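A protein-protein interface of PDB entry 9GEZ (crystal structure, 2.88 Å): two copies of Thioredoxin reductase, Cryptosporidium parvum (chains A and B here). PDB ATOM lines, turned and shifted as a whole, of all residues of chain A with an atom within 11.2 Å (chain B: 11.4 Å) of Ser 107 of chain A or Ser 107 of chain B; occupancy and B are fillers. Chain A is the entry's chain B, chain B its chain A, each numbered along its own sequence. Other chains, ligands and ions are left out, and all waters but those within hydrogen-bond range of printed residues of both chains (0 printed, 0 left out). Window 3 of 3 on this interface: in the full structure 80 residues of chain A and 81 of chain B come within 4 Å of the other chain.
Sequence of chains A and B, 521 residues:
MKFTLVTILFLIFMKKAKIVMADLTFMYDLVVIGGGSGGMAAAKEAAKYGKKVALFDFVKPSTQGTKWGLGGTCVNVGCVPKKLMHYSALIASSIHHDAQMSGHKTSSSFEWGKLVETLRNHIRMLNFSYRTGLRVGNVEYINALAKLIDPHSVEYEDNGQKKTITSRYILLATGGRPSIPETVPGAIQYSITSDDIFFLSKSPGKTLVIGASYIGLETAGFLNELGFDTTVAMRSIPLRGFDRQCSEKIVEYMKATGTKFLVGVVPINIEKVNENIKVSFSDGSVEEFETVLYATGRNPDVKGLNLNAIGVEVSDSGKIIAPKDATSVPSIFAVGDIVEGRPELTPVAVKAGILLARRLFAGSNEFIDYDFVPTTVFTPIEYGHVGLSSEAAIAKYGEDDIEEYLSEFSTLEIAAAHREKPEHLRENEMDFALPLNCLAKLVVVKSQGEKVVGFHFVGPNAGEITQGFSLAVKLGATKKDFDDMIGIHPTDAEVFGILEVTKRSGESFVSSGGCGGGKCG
The backbone carbonyl oxygen (O) of Gly 103 of chain B lies within hydrogen-bond range of the backbone NH (N) of Glu 111 of chain A (2.6 Å). N of Glu 111 of chain B sits at hydrogen-bond distance from O of Gly 103 of chain A (2.8 Å). N of Lys 105 of chain B sits at hydrogen-bond distance from O of Ser 109 of chain A (2.8 Å). N of Lys 105 of chain A sits at hydrogen-bond distance from O of Ser 109 of chain B, at 3.0 Å. The side-chain hydroxyl (OG) of Ser 108 of chain B is in hydrogen-bond range of the backbone carbonyl oxygen (O) of Lys 105 of chain A (2.9 Å). O of Ser 107 of chain B sits at hydrogen-bond distance from N of Ser 107 of chain A, 3.0 Å away.
N of His 104 of chain B is in hydrogen-bond range of O of Ala 99 of chain B (2.6 Å). N of Ala 99 of chain A is in hydrogen-bond range of O of Ser 94 of chain A. O of Ile 91 of chain A is in hydrogen-bond range of OG of Ser 94 of chain A, 2.7 Å away. The backbone carbonyl oxygen (O) of Ile 91 of chain B sits at hydrogen-bond distance from the side-chain hydroxyl (OG) of Ser 94 of chain B (2.7 Å). O of Ala 99 of chain A is in hydrogen-bond range of N of His 104 of chain A (2.8 Å). The backbone carbonyl oxygen (O) of Ser 94 of chain B is in hydrogen-bond range of the backbone NH (N) of Ala 99 of chain B.
CD1 of Ile 91 of chain A touches N of Ala 99 of chain B (3.96 Å). Ala 92 of chain A touches His 104 of chain B (CB to NE2, 3.8 Å). Phe 110 of chain B touches Gly 103 of chain A. His 104 of chain A touches Ile 91 of chain B. Ser 108 of chain B touches His 104 of chain A. His 104 of chain A touches Ser 109 of chain B. ND1 of His 104 of chain A touches CD1 of Phe 110 of chain B, 3.6 Å away. Thr 106 of chain A touches Ser 107 of chain B. O of Ser 107 of chain A touches O of Lys 105 of chain B, 3.8 Å away. Ser 109 of chain A touches His 104 of chain B (O to C, 3.7 Å).
Ser 107 of chain B touches two residues of chain A. Of chain B, only Ile 95 (3.4 Å), Ser 107 (3.3 Å) and Ser 108 (2.8 Å) come within 4 Å of Thr 106 of chain A. Ser 109 of chain A touches two residues of chain B. Ser 109 of chain B touches just these residues of chain A: Gly 103 (3.95 Å), His 104 (3.7 Å) and Lys 105 (3.0 Å). Printed residues of chain A within 4 Å of Ile 91 of chain B: Ala 99 and His 104. Of the printed residues of chain B, Glu 111 of chain A touches Gly 103 (2.6 Å). Printed residues of chain A within 4 Å of Phe 110 of chain B: Gly 103 (3.4 Å) and His 104 (3.6 Å). Printed residues of chain B within 4 Å of Ser 108 of chain A: His 104 (3.995 Å), Lys 105 (3.1 Å) and Thr 106 (3.8 Å). Ser 94 of chain B touches none of the printed residues of chain A. The nearest residue of chain B that does not touch Ser 107 of chain A is Ser 108 of chain B (5.1 Å). The nearest residue of chain A that does not touch Ser 107 of chain B is Lys 105 of chain A (4.1 Å). The nearest printed residue of chain A that does not touch Ala 92 of chain B is Ala 99 of chain A (7.4 Å).
Printed residues of chain B that touch a printed residue of chain A: Ile 91, Ala 92, Ile 95, Asp 98, Ala 99, Gly 103, His 104, Lys 105, Thr 106, Ser 107, Ser 108, Ser 109, Phe 110 and Glu 111. Hydrophobic or aromatic side chains of chain B that line the printed part of chain A: Ile 91, Ala 92, Ile 95, His 104 and Phe 110. Printed residues of chain A that touch a printed residue of chain B: Ile 91, Ala 92, Ile 95, Ala 99, Gly 103, His 104, Lys 105, Thr 106, Ser 107, Ser 108, Ser 109, Phe 110 and Glu 111. Hydrophobic or aromatic side chains of chain A that line the printed part of chain B: Ile 91, Ala 92, Ile 95, His 104 and Phe 110. Among the printed residues, no Asp or Glu carboxylate lies within 4 Å of a Lys or Arg side-chain nitrogen of the other chain.
Ile 91 of chain A touches His 104 of chain B, and with the chains exchanged His 104 of chain A touches Ile 91 of chain B. Gly 103 of chain A touches Phe 110 of chain B, and with the chains exchanged Phe 110 of chain A touches Gly 103 of chain B. Lys 105 of chain A touches Ser 108 of chain B, and with the chains exchanged Ser 108 of chain A touches Lys 105 of chain B. Thr 106 of chain A touches Ser 108 of chain B, and with the chains exchanged Ser 108 of chain A touches Thr 106 of chain B. Positions printed for both chains: 91, 92, 94, 95, 96, 99, 100, 103, 104, 105, 106, 107, 108, 109, 110 and 111. Of the 30 pairs that touch across the chains among the printed residues, 27 have their exchanged pair printed and touching as well.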
ATOM      1  N   ILE A  91      18.366  29.462  10.410  1.00  0.00           N
ATOM      2  CA  ILE A  91      19.047  29.442  11.737  1.00  0.00           C
ATOM      3  C   ILE A  91      20.546  29.118  11.539  1.00  0.00           C
ATOM      4  O   ILE A  91      21.376  29.957  11.975  1.00  0.00           O
ATOM      5  CB  ILE A  91      18.404  28.447  12.719  1.00  0.00           C
ATOM      6  CG1 ILE A  91      17.157  29.025  13.379  1.00  0.00           C
ATOM      7  CG2 ILE A  91      19.434  27.969  13.743  1.00  0.00           C
ATOM      8  CD1 ILE A  91      16.648  28.191  14.507  1.00  0.00           C
ATOM      9  N   ALA A  92      20.875  27.973  10.907  1.00  0.00           N
ATOM     10  CA  ALA A  92      22.257  27.447  10.766  1.00  0.00           C
ATOM     11  C   ALA A  92      23.200  28.530  10.226  1.00  0.00           C
ATOM     12  O   ALA A  92      24.320  28.638  10.766  1.00  0.00           O
ATOM     13  CB  ALA A  92      22.267  26.215   9.899  1.00  0.00           C
ATOM     14  N   SER A  94      22.876  31.973  10.423  1.00  0.00           N
ATOM     15  CA  SER A  94      23.047  33.075  11.398  1.00  0.00           C
ATOM     16  C   SER A  94      24.104  32.603  12.386  1.00  0.00           C
ATOM     17  O   SER A  94      25.199  33.210  12.432  1.00  0.00           O
ATOM     18  CB  SER A  94      21.744  33.455  12.038  1.00  0.00           C
ATOM     19  OG  SER A  94      21.336  32.462  12.943  1.00  0.00           O
ATOM     20  N   ILE A  95      23.853  31.446  12.997  1.00  0.00           N
ATOM     21  CA  ILE A  95      24.823  30.736  13.881  1.00  0.00           C
ATOM     22  C   ILE A  95      26.241  30.860  13.300  1.00  0.00           C
ATOM     23  O   ILE A  95      27.114  31.350  14.047  1.00  0.00           O
ATOM     24  CB  ILE A  95      24.408  29.273  14.099  1.00  0.00           C
ATOM     25  CG1 ILE A  95      23.220  29.179  15.067  1.00  0.00           C
ATOM     26  CG2 ILE A  95      25.604  28.463  14.560  1.00  0.00           C
ATOM     27  CD1 ILE A  95      22.999  27.801  15.669  1.00  0.00           C
ATOM     28  N   HIS A  96      26.462  30.446  12.042  1.00  0.00           N
ATOM     29  CA  HIS A  96      27.799  30.330  11.390  1.00  0.00           C
ATOM     30  C   HIS A  96      28.341  31.688  10.914  1.00  0.00           C
ATOM     31  O   HIS A  96      29.575  31.845  10.880  1.00  0.00           O
ATOM     32  CB  HIS A  96      27.755  29.369  10.196  1.00  0.00           C
ATOM     33  CG  HIS A  96      28.989  29.464   9.363  1.00  0.00           C
ATOM     34  ND1 HIS A  96      28.999  30.068   8.122  1.00  0.00           N
ATOM     35  CD2 HIS A  96      30.263  29.095   9.620  1.00  0.00           C
ATOM     36  CE1 HIS A  96      30.225  30.038   7.641  1.00  0.00           C
ATOM     37  NE2 HIS A  96      31.016  29.451   8.543  1.00  0.00           N
ATOM     38  N   HIS A  97      27.472  32.606  10.478  1.00  0.00           N
ATOM     39  CA  HIS A  97      27.877  33.914   9.902  1.00  0.00           C
ATOM     40  C   HIS A  97      27.739  35.034  10.938  1.00  0.00           C
ATOM     41  O   HIS A  97      28.667  35.868  11.015  1.00  0.00           O
ATOM     42  CB  HIS A  97      27.067  34.217   8.647  1.00  0.00           C
ATOM     43  CG  HIS A  97      27.278  33.258   7.523  1.00  0.00           C
ATOM     44  ND1 HIS A  97      28.360  33.345   6.655  1.00  0.00           N
ATOM     45  CD2 HIS A  97      26.522  32.228   7.091  1.00  0.00           C
ATOM     46  CE1 HIS A  97      28.269  32.393   5.753  1.00  0.00           C
ATOM     47  NE2 HIS A  97      27.139  31.696   6.002  1.00  0.00           N
ATOM     48  N   ALA A  99      26.067  35.118  14.596  1.00  0.00           N
ATOM     49  CA  ALA A  99      26.203  34.920  16.052  1.00  0.00           C
ATOM     50  C   ALA A  99      27.371  35.680  16.675  1.00  0.00           C
ATOM     51  O   ALA A  99      27.140  36.453  17.622  1.00  0.00           O
ATOM     52  CB  ALA A  99      26.396  33.453  16.350  1.00  0.00           C
ATOM     53  N   GLN A 100      28.571  35.456  16.132  1.00  0.00           N
ATOM     54  CA  GLN A 100      29.894  35.865  16.685  1.00  0.00           C
ATOM     55  C   GLN A 100      29.980  37.387  16.639  1.00  0.00           C
ATOM     56  O   GLN A 100      30.442  37.979  17.630  1.00  0.00           O
ATOM     57  CB  GLN A 100      31.030  35.277  15.836  1.00  0.00           C
ATOM     58  CG  GLN A 100      32.429  35.744  16.225  1.00  0.00           C
ATOM     59  CD  GLN A 100      33.065  34.831  17.244  1.00  0.00           C
ATOM     60  OE1 GLN A 100      33.808  33.915  16.902  1.00  0.00           O
ATOM     61  NE2 GLN A 100      32.763  35.088  18.507  1.00  0.00           N
ATOM     62  N   GLY A 103      28.321  39.097  19.072  1.00  0.00           N
ATOM     63  CA  GLY A 103      29.076  38.892  20.321  1.00  0.00           C
ATOM     64  C   GLY A 103      28.683  37.601  20.994  1.00  0.00           C
ATOM     65  O   GLY A 103      28.963  37.482  22.220  1.00  0.00           O
ATOM     66  N   HIS A 104      28.089  36.668  20.229  1.00  0.00           N
ATOM     67  CA  HIS A 104      27.674  35.312  20.681  1.00  0.00           C
ATOM     68  C   HIS A 104      28.662  34.280  20.134  1.00  0.00           C
ATOM     69  O   HIS A 104      28.566  34.000  18.913  1.00  0.00           O
ATOM     70  CB  HIS A 104      26.275  34.935  20.158  1.00  0.00           C
ATOM     71  CG  HIS A 104      25.176  35.909  20.415  1.00  0.00           C
ATOM     72  ND1 HIS A 104      24.589  36.027  21.659  1.00  0.00           N
ATOM     73  CD2 HIS A 104      24.506  36.741  19.588  1.00  0.00           C
ATOM     74  CE1 HIS A 104      23.612  36.909  21.594  1.00  0.00           C
ATOM     75  NE2 HIS A 104      23.542  37.361  20.336  1.00  0.00           N
ATOM     76  N   LYS A 105      29.537  33.708  20.977  1.00  0.00           N
ATOM     77  CA  LYS A 105      30.457  32.611  20.558  1.00  0.00           C
ATOM     78  C   LYS A 105      29.752  31.264  20.779  1.00  0.00           C
ATOM     79  O   LYS A 105      29.205  31.056  21.878  1.00  0.00           O
ATOM     80  CB  LYS A 105      31.800  32.732  21.280  1.00  0.00           C
ATOM     81  CG  LYS A 105      32.893  31.790  20.787  1.00  0.00           C
ATOM     82  CD  LYS A 105      33.318  32.025  19.344  1.00  0.00           C
ATOM     83  CE  LYS A 105      34.257  30.959  18.813  1.00  0.00           C
ATOM     84  NZ  LYS A 105      35.685  31.332  18.959  1.00  0.00           N
ATOM     85  N   THR A 106      29.781  30.389  19.764  1.00  0.00           N
ATOM     86  CA  THR A 106      28.796  29.288  19.545  1.00  0.00           C
ATOM     87  C   THR A 106      29.493  28.035  19.006  1.00  0.00           C
ATOM     88  O   THR A 106      30.152  28.126  17.955  1.00  0.00           O
ATOM     89  CB  THR A 106      27.726  29.717  18.530  1.00  0.00           C
ATOM     90  OG1 THR A 106      28.385  30.558  17.584  1.00  0.00           O
ATOM     91  CG2 THR A 106      26.579  30.530  19.085  1.00  0.00           C
ATOM     92  N   SER A 107      29.381  26.914  19.722  1.00  0.00           N
ATOM     93  CA  SER A 107      29.630  25.552  19.188  1.00  0.00           C
ATOM     94  C   SER A 107      28.272  24.974  18.786  1.00  0.00           C
ATOM     95  O   SER A 107      27.254  25.319  19.415  1.00  0.00           O
ATOM     96  CB  SER A 107      30.371  24.644  20.150  1.00  0.00           C
ATOM     97  OG  SER A 107      29.507  23.653  20.695  1.00  0.00           O
ATOM     98  N   SER A 108      28.268  24.177  17.724  1.00  0.00           N
ATOM     99  CA  SER A 108      27.035  23.648  17.110  1.00  0.00           C
ATOM    100  C   SER A 108      27.385  22.467  16.203  1.00  0.00           C
ATOM    101  O   SER A 108      28.187  22.629  15.273  1.00  0.00           O
ATOM    102  CB  SER A 108      26.317  24.762  16.387  1.00  0.00           C
ATOM    103  OG  SER A 108      25.058  24.347  15.868  1.00  0.00           O
ATOM    104  N   SER A 109      26.813  21.313  16.517  1.00  0.00           N
ATOM    105  CA  SER A 109      26.687  20.144  15.611  1.00  0.00           C
ATOM    106  C   SER A 109      25.198  19.893  15.434  1.00  0.00           C
ATOM    107  O   SER A 109      24.438  20.271  16.340  1.00  0.00           O
ATOM    108  CB  SER A 109      27.435  18.902  16.102  1.00  0.00           C
ATOM    109  OG  SER A 109      26.651  18.147  17.004  1.00  0.00           O
ATOM    110  N   PHE A 110      24.823  19.255  14.321  1.00  0.00           N
ATOM    111  CA  PHE A 110      23.427  19.104  13.823  1.00  0.00           C
ATOM    112  C   PHE A 110      22.951  17.639  13.807  1.00  0.00           C
ATOM    113  O   PHE A 110      23.708  16.786  13.333  1.00  0.00           O
ATOM    114  CB  PHE A 110      23.366  19.685  12.413  1.00  0.00           C
ATOM    115  CG  PHE A 110      22.068  19.385  11.716  1.00  0.00           C
ATOM    116  CD1 PHE A 110      20.908  20.060  12.074  1.00  0.00           C
ATOM    117  CD2 PHE A 110      22.003  18.394  10.749  1.00  0.00           C
ATOM    118  CE1 PHE A 110      19.713  19.762  11.460  1.00  0.00           C
ATOM    119  CE2 PHE A 110      20.804  18.103  10.131  1.00  0.00           C
ATOM    120  CZ  PHE A 110      19.666  18.798  10.478  1.00  0.00           C
ATOM    121  N   GLU A 111      21.693  17.372  14.198  1.00  0.00           N
ATOM    122  CA  GLU A 111      21.073  16.008  14.187  1.00  0.00           C
ATOM    123  C   GLU A 111      19.808  15.965  13.303  1.00  0.00           C
ATOM    124  O   GLU A 111      18.702  16.219  13.782  1.00  0.00           O
ATOM    125  CB  GLU A 111      20.786  15.562  15.620  1.00  0.00           C
ATOM    126  CG  GLU A 111      22.021  15.493  16.495  1.00  0.00           C
ATOM    127  CD  GLU A 111      22.929  14.310  16.232  1.00  0.00           C
ATOM    128  OE1 GLU A 111      23.521  13.804  17.209  1.00  0.00           O
ATOM    129  OE2 GLU A 111      23.048  13.904  15.064  1.00  0.00           O
ATOM    130  N   ILE B  91      18.621  36.820  17.419  1.00  0.00           N
ATOM    131  CA  ILE B  91      19.555  35.654  17.324  1.00  0.00           C
ATOM    132  C   ILE B  91      19.490  34.847  18.632  1.00  0.00           C
ATOM    133  O   ILE B  91      19.165  33.641  18.566  1.00  0.00           O
ATOM    134  CB  ILE B  91      21.016  36.073  17.034  1.00  0.00           C
ATOM    135  CG1 ILE B  91      21.237  36.455  15.568  1.00  0.00           C
ATOM    136  CG2 ILE B  91      21.946  34.946  17.473  1.00  0.00           C
ATOM    137  CD1 ILE B  91      22.668  36.418  15.112  1.00  0.00           C
ATOM    138  N   ALA B  92      19.797  35.490  19.770  1.00  0.00           N
ATOM    139  CA  ALA B  92      19.951  34.855  21.104  1.00  0.00           C
ATOM    140  C   ALA B  92      18.700  34.065  21.449  1.00  0.00           C
ATOM    141  O   ALA B  92      18.866  32.965  22.005  1.00  0.00           O
ATOM    142  CB  ALA B  92      20.206  35.875  22.183  1.00  0.00           C
ATOM    143  N   SER B  94      16.489  32.538  19.287  1.00  0.00           N
ATOM    144  CA  SER B  94      16.394  31.345  18.423  1.00  0.00           C
ATOM    145  C   SER B  94      17.364  30.339  19.041  1.00  0.00           C
ATOM    146  O   SER B  94      16.896  29.274  19.479  1.00  0.00           O
ATOM    147  CB  SER B  94      16.681  31.690  16.983  1.00  0.00           C
ATOM    148  OG  SER B  94      18.065  31.945  16.804  1.00  0.00           O
ATOM    149  N   ILE B  95      18.626  30.725  19.209  1.00  0.00           N
ATOM    150  CA  ILE B  95      19.654  29.918  19.946  1.00  0.00           C
ATOM    151  C   ILE B  95      19.024  29.203  21.157  1.00  0.00           C
ATOM    152  O   ILE B  95      19.154  27.970  21.202  1.00  0.00           O
ATOM    153  CB  ILE B  95      20.861  30.781  20.365  1.00  0.00           C
ATOM    154  CG1 ILE B  95      21.778  31.066  19.163  1.00  0.00           C
ATOM    155  CG2 ILE B  95      21.590  30.116  21.511  1.00  0.00           C
ATOM    156  CD1 ILE B  95      23.261  31.171  19.464  1.00  0.00           C
ATOM    157  N   HIS B  96      18.359  29.944  22.070  1.00  0.00           N
ATOM    158  CA  HIS B  96      17.824  29.446  23.371  1.00  0.00           C
ATOM    159  C   HIS B  96      16.508  28.677  23.209  1.00  0.00           C
ATOM    160  O   HIS B  96      16.256  27.745  24.019  1.00  0.00           O
ATOM    161  CB  HIS B  96      17.602  30.579  24.382  1.00  0.00           C
ATOM    162  CG  HIS B  96      16.805  30.122  25.563  1.00  0.00           C
ATOM    163  ND1 HIS B  96      15.464  30.478  25.741  1.00  0.00           N
ATOM    164  CD2 HIS B  96      17.109  29.275  26.570  1.00  0.00           C
ATOM    165  CE1 HIS B  96      14.992  29.887  26.817  1.00  0.00           C
ATOM    166  NE2 HIS B  96      15.984  29.143  27.342  1.00  0.00           N
ATOM    167  N   ASP B  98      15.012  27.747  19.829  1.00  0.00           N
ATOM    168  CA  ASP B  98      14.787  27.124  18.497  1.00  0.00           C
ATOM    169  C   ASP B  98      15.943  26.164  18.194  1.00  0.00           C
ATOM    170  O   ASP B  98      15.701  24.975  18.107  1.00  0.00           O
ATOM    171  CB  ASP B  98      14.551  28.219  17.457  1.00  0.00           C
ATOM    172  CG  ASP B  98      13.327  29.117  17.696  1.00  0.00           C
ATOM    173  OD1 ASP B  98      12.364  28.717  18.363  1.00  0.00           O
ATOM    174  OD2 ASP B  98      13.335  30.237  17.202  1.00  0.00           O
ATOM    175  N   ALA B  99      17.175  26.636  18.116  1.00  0.00           N
ATOM    176  CA  ALA B  99      18.351  25.844  17.673  1.00  0.00           C
ATOM    177  C   ALA B  99      18.348  24.312  17.814  1.00  0.00           C
ATOM    178  O   ALA B  99      18.639  23.633  16.821  1.00  0.00           O
ATOM    179  CB  ALA B  99      19.566  26.243  18.456  1.00  0.00           C
ATOM    180  N   GLN B 100      17.985  23.796  18.985  1.00  0.00           N
ATOM    181  CA  GLN B 100      17.914  22.332  19.295  1.00  0.00           C
ATOM    182  C   GLN B 100      16.680  21.702  18.622  1.00  0.00           C
ATOM    183  O   GLN B 100      16.810  20.585  18.096  1.00  0.00           O
ATOM    184  CB  GLN B 100      17.858  22.132  20.812  1.00  0.00           C
ATOM    185  CG  GLN B 100      17.582  20.707  21.263  1.00  0.00           C
ATOM    186  CD  GLN B 100      18.844  19.944  21.586  1.00  0.00           C
ATOM    187  OE1 GLN B 100      19.219  19.793  22.748  1.00  0.00           O
ATOM    188  NE2 GLN B 100      19.507  19.448  20.548  1.00  0.00           N
ATOM    189  N   GLY B 103      17.148  20.850  15.378  1.00  0.00           N
ATOM    190  CA  GLY B 103      18.140  19.758  15.376  1.00  0.00           C
ATOM    191  C   GLY B 103      19.575  20.257  15.448  1.00  0.00           C
ATOM    192  O   GLY B 103      20.440  19.523  14.962  1.00  0.00           O
ATOM    193  N   HIS B 104      19.813  21.473  15.964  1.00  0.00           N
ATOM    194  CA  HIS B 104      21.150  22.134  16.091  1.00  0.00           C
ATOM    195  C   HIS B 104      21.551  22.240  17.574  1.00  0.00           C
ATOM    196  O   HIS B 104      20.976  23.129  18.271  1.00  0.00           O
ATOM    197  CB  HIS B 104      21.160  23.561  15.481  1.00  0.00           C
ATOM    198  CG  HIS B 104      20.924  23.614  14.013  1.00  0.00           C
ATOM    199  ND1 HIS B 104      21.763  22.988  13.089  1.00  0.00           N
ATOM    200  CD2 HIS B 104      19.915  24.174  13.310  1.00  0.00           C
ATOM    201  CE1 HIS B 104      21.268  23.169  11.872  1.00  0.00           C
ATOM    202  NE2 HIS B 104      20.136  23.916  11.978  1.00  0.00           N
ATOM    203  N   LYS B 105      22.490  21.398  18.032  1.00  0.00           N
ATOM    204  CA  LYS B 105      22.880  21.297  19.464  1.00  0.00           C
ATOM    205  C   LYS B 105      24.059  22.257  19.728  1.00  0.00           C
ATOM    206  O   LYS B 105      25.041  22.210  18.932  1.00  0.00           O
ATOM    207  CB  LYS B 105      23.199  19.838  19.811  1.00  0.00           C
ATOM    208  CG  LYS B 105      23.454  19.552  21.291  1.00  0.00           C
ATOM    209  CD  LYS B 105      22.267  19.836  22.194  1.00  0.00           C
ATOM    210  CE  LYS B 105      22.636  20.372  23.561  1.00  0.00           C
ATOM    211  NZ  LYS B 105      22.545  19.306  24.581  1.00  0.00           N
ATOM    212  N   THR B 106      23.976  23.064  20.810  1.00  0.00           N
ATOM    213  CA  THR B 106      24.668  24.372  20.938  1.00  0.00           C
ATOM    214  C   THR B 106      25.146  24.680  22.368  1.00  0.00           C
ATOM    215  O   THR B 106      24.338  24.594  23.309  1.00  0.00           O
ATOM    216  CB  THR B 106      23.744  25.531  20.546  1.00  0.00           C
ATOM    217  OG1 THR B 106      22.423  25.166  20.965  1.00  0.00           O
ATOM    218  CG2 THR B 106      23.785  25.872  19.072  1.00  0.00           C
ATOM    219  N   SER B 107      26.415  25.087  22.504  1.00  0.00           N
ATOM    220  CA  SER B 107      26.917  25.970  23.584  1.00  0.00           C
ATOM    221  C   SER B 107      26.986  27.373  22.993  1.00  0.00           C
ATOM    222  O   SER B 107      27.208  27.484  21.769  1.00  0.00           O
ATOM    223  CB  SER B 107      28.274  25.527  24.123  1.00  0.00           C
ATOM    224  OG  SER B 107      29.312  26.431  23.745  1.00  0.00           O
ATOM    225  N   SER B 108      26.818  28.398  23.821  1.00  0.00           N
ATOM    226  CA  SER B 108      27.004  29.803  23.399  1.00  0.00           C
ATOM    227  C   SER B 108      27.090  30.697  24.630  1.00  0.00           C
ATOM    228  O   SER B 108      26.177  30.610  25.472  1.00  0.00           O
ATOM    229  CB  SER B 108      25.906  30.251  22.469  1.00  0.00           C
ATOM    230  OG  SER B 108      26.326  31.392  21.735  1.00  0.00           O
ATOM    231  N   SER B 109      28.162  31.481  24.751  1.00  0.00           N
ATOM    232  CA  SER B 109      28.287  32.547  25.769  1.00  0.00           C
ATOM    233  C   SER B 109      28.336  33.884  25.040  1.00  0.00           C
ATOM    234  O   SER B 109      28.769  33.902  23.885  1.00  0.00           O
ATOM    235  CB  SER B 109      29.480  32.338  26.706  1.00  0.00           C
ATOM    236  OG  SER B 109      30.663  32.967  26.225  1.00  0.00           O
ATOM    237  N   PHE B 110      27.915  34.939  25.736  1.00  0.00           N
ATOM    238  CA  PHE B 110      27.727  36.305  25.197  1.00  0.00           C
ATOM    239  C   PHE B 110      28.735  37.297  25.795  1.00  0.00           C
ATOM    240  O   PHE B 110      28.844  37.365  27.030  1.00  0.00           O
ATOM    241  CB  PHE B 110      26.314  36.772  25.507  1.00  0.00           C
ATOM    242  CG  PHE B 110      26.085  38.202  25.124  1.00  0.00           C
ATOM    243  CD1 PHE B 110      25.892  38.550  23.802  1.00  0.00           C
ATOM    244  CD2 PHE B 110      26.109  39.208  26.076  1.00  0.00           C
ATOM    245  CE1 PHE B 110      25.651  39.869  23.446  1.00  0.00           C
ATOM    246  CE2 PHE B 110      25.897  40.528  25.715  1.00  0.00           C
ATOM    247  CZ  PHE B 110      25.657  40.853  24.402  1.00  0.00           C
ATOM    248  N   GLU B 111      29.420  38.060  24.934  1.00  0.00           N
ATOM    249  CA  GLU B 111      30.329  39.170  25.323  1.00  0.00           C
ATOM    250  C   GLU B 111      29.854  40.475  24.674  1.00  0.00           C
ATOM    251  O   GLU B 111      30.279  40.803  23.512  1.00  0.00           O
ATOM    252  CB  GLU B 111      31.784  38.832  25.004  1.00  0.00           C
ATOM    253  CG  GLU B 111      32.327  37.684  25.871  1.00  0.00           C
ATOM    254  CD  GLU B 111      32.443  37.948  27.377  1.00  0.00           C
ATOM    255  OE1 GLU B 111      31.717  37.288  28.163  1.00  0.00           O
ATOM    256  OE2 GLU B 111      33.244  38.823  27.765  1.00  0.00           O
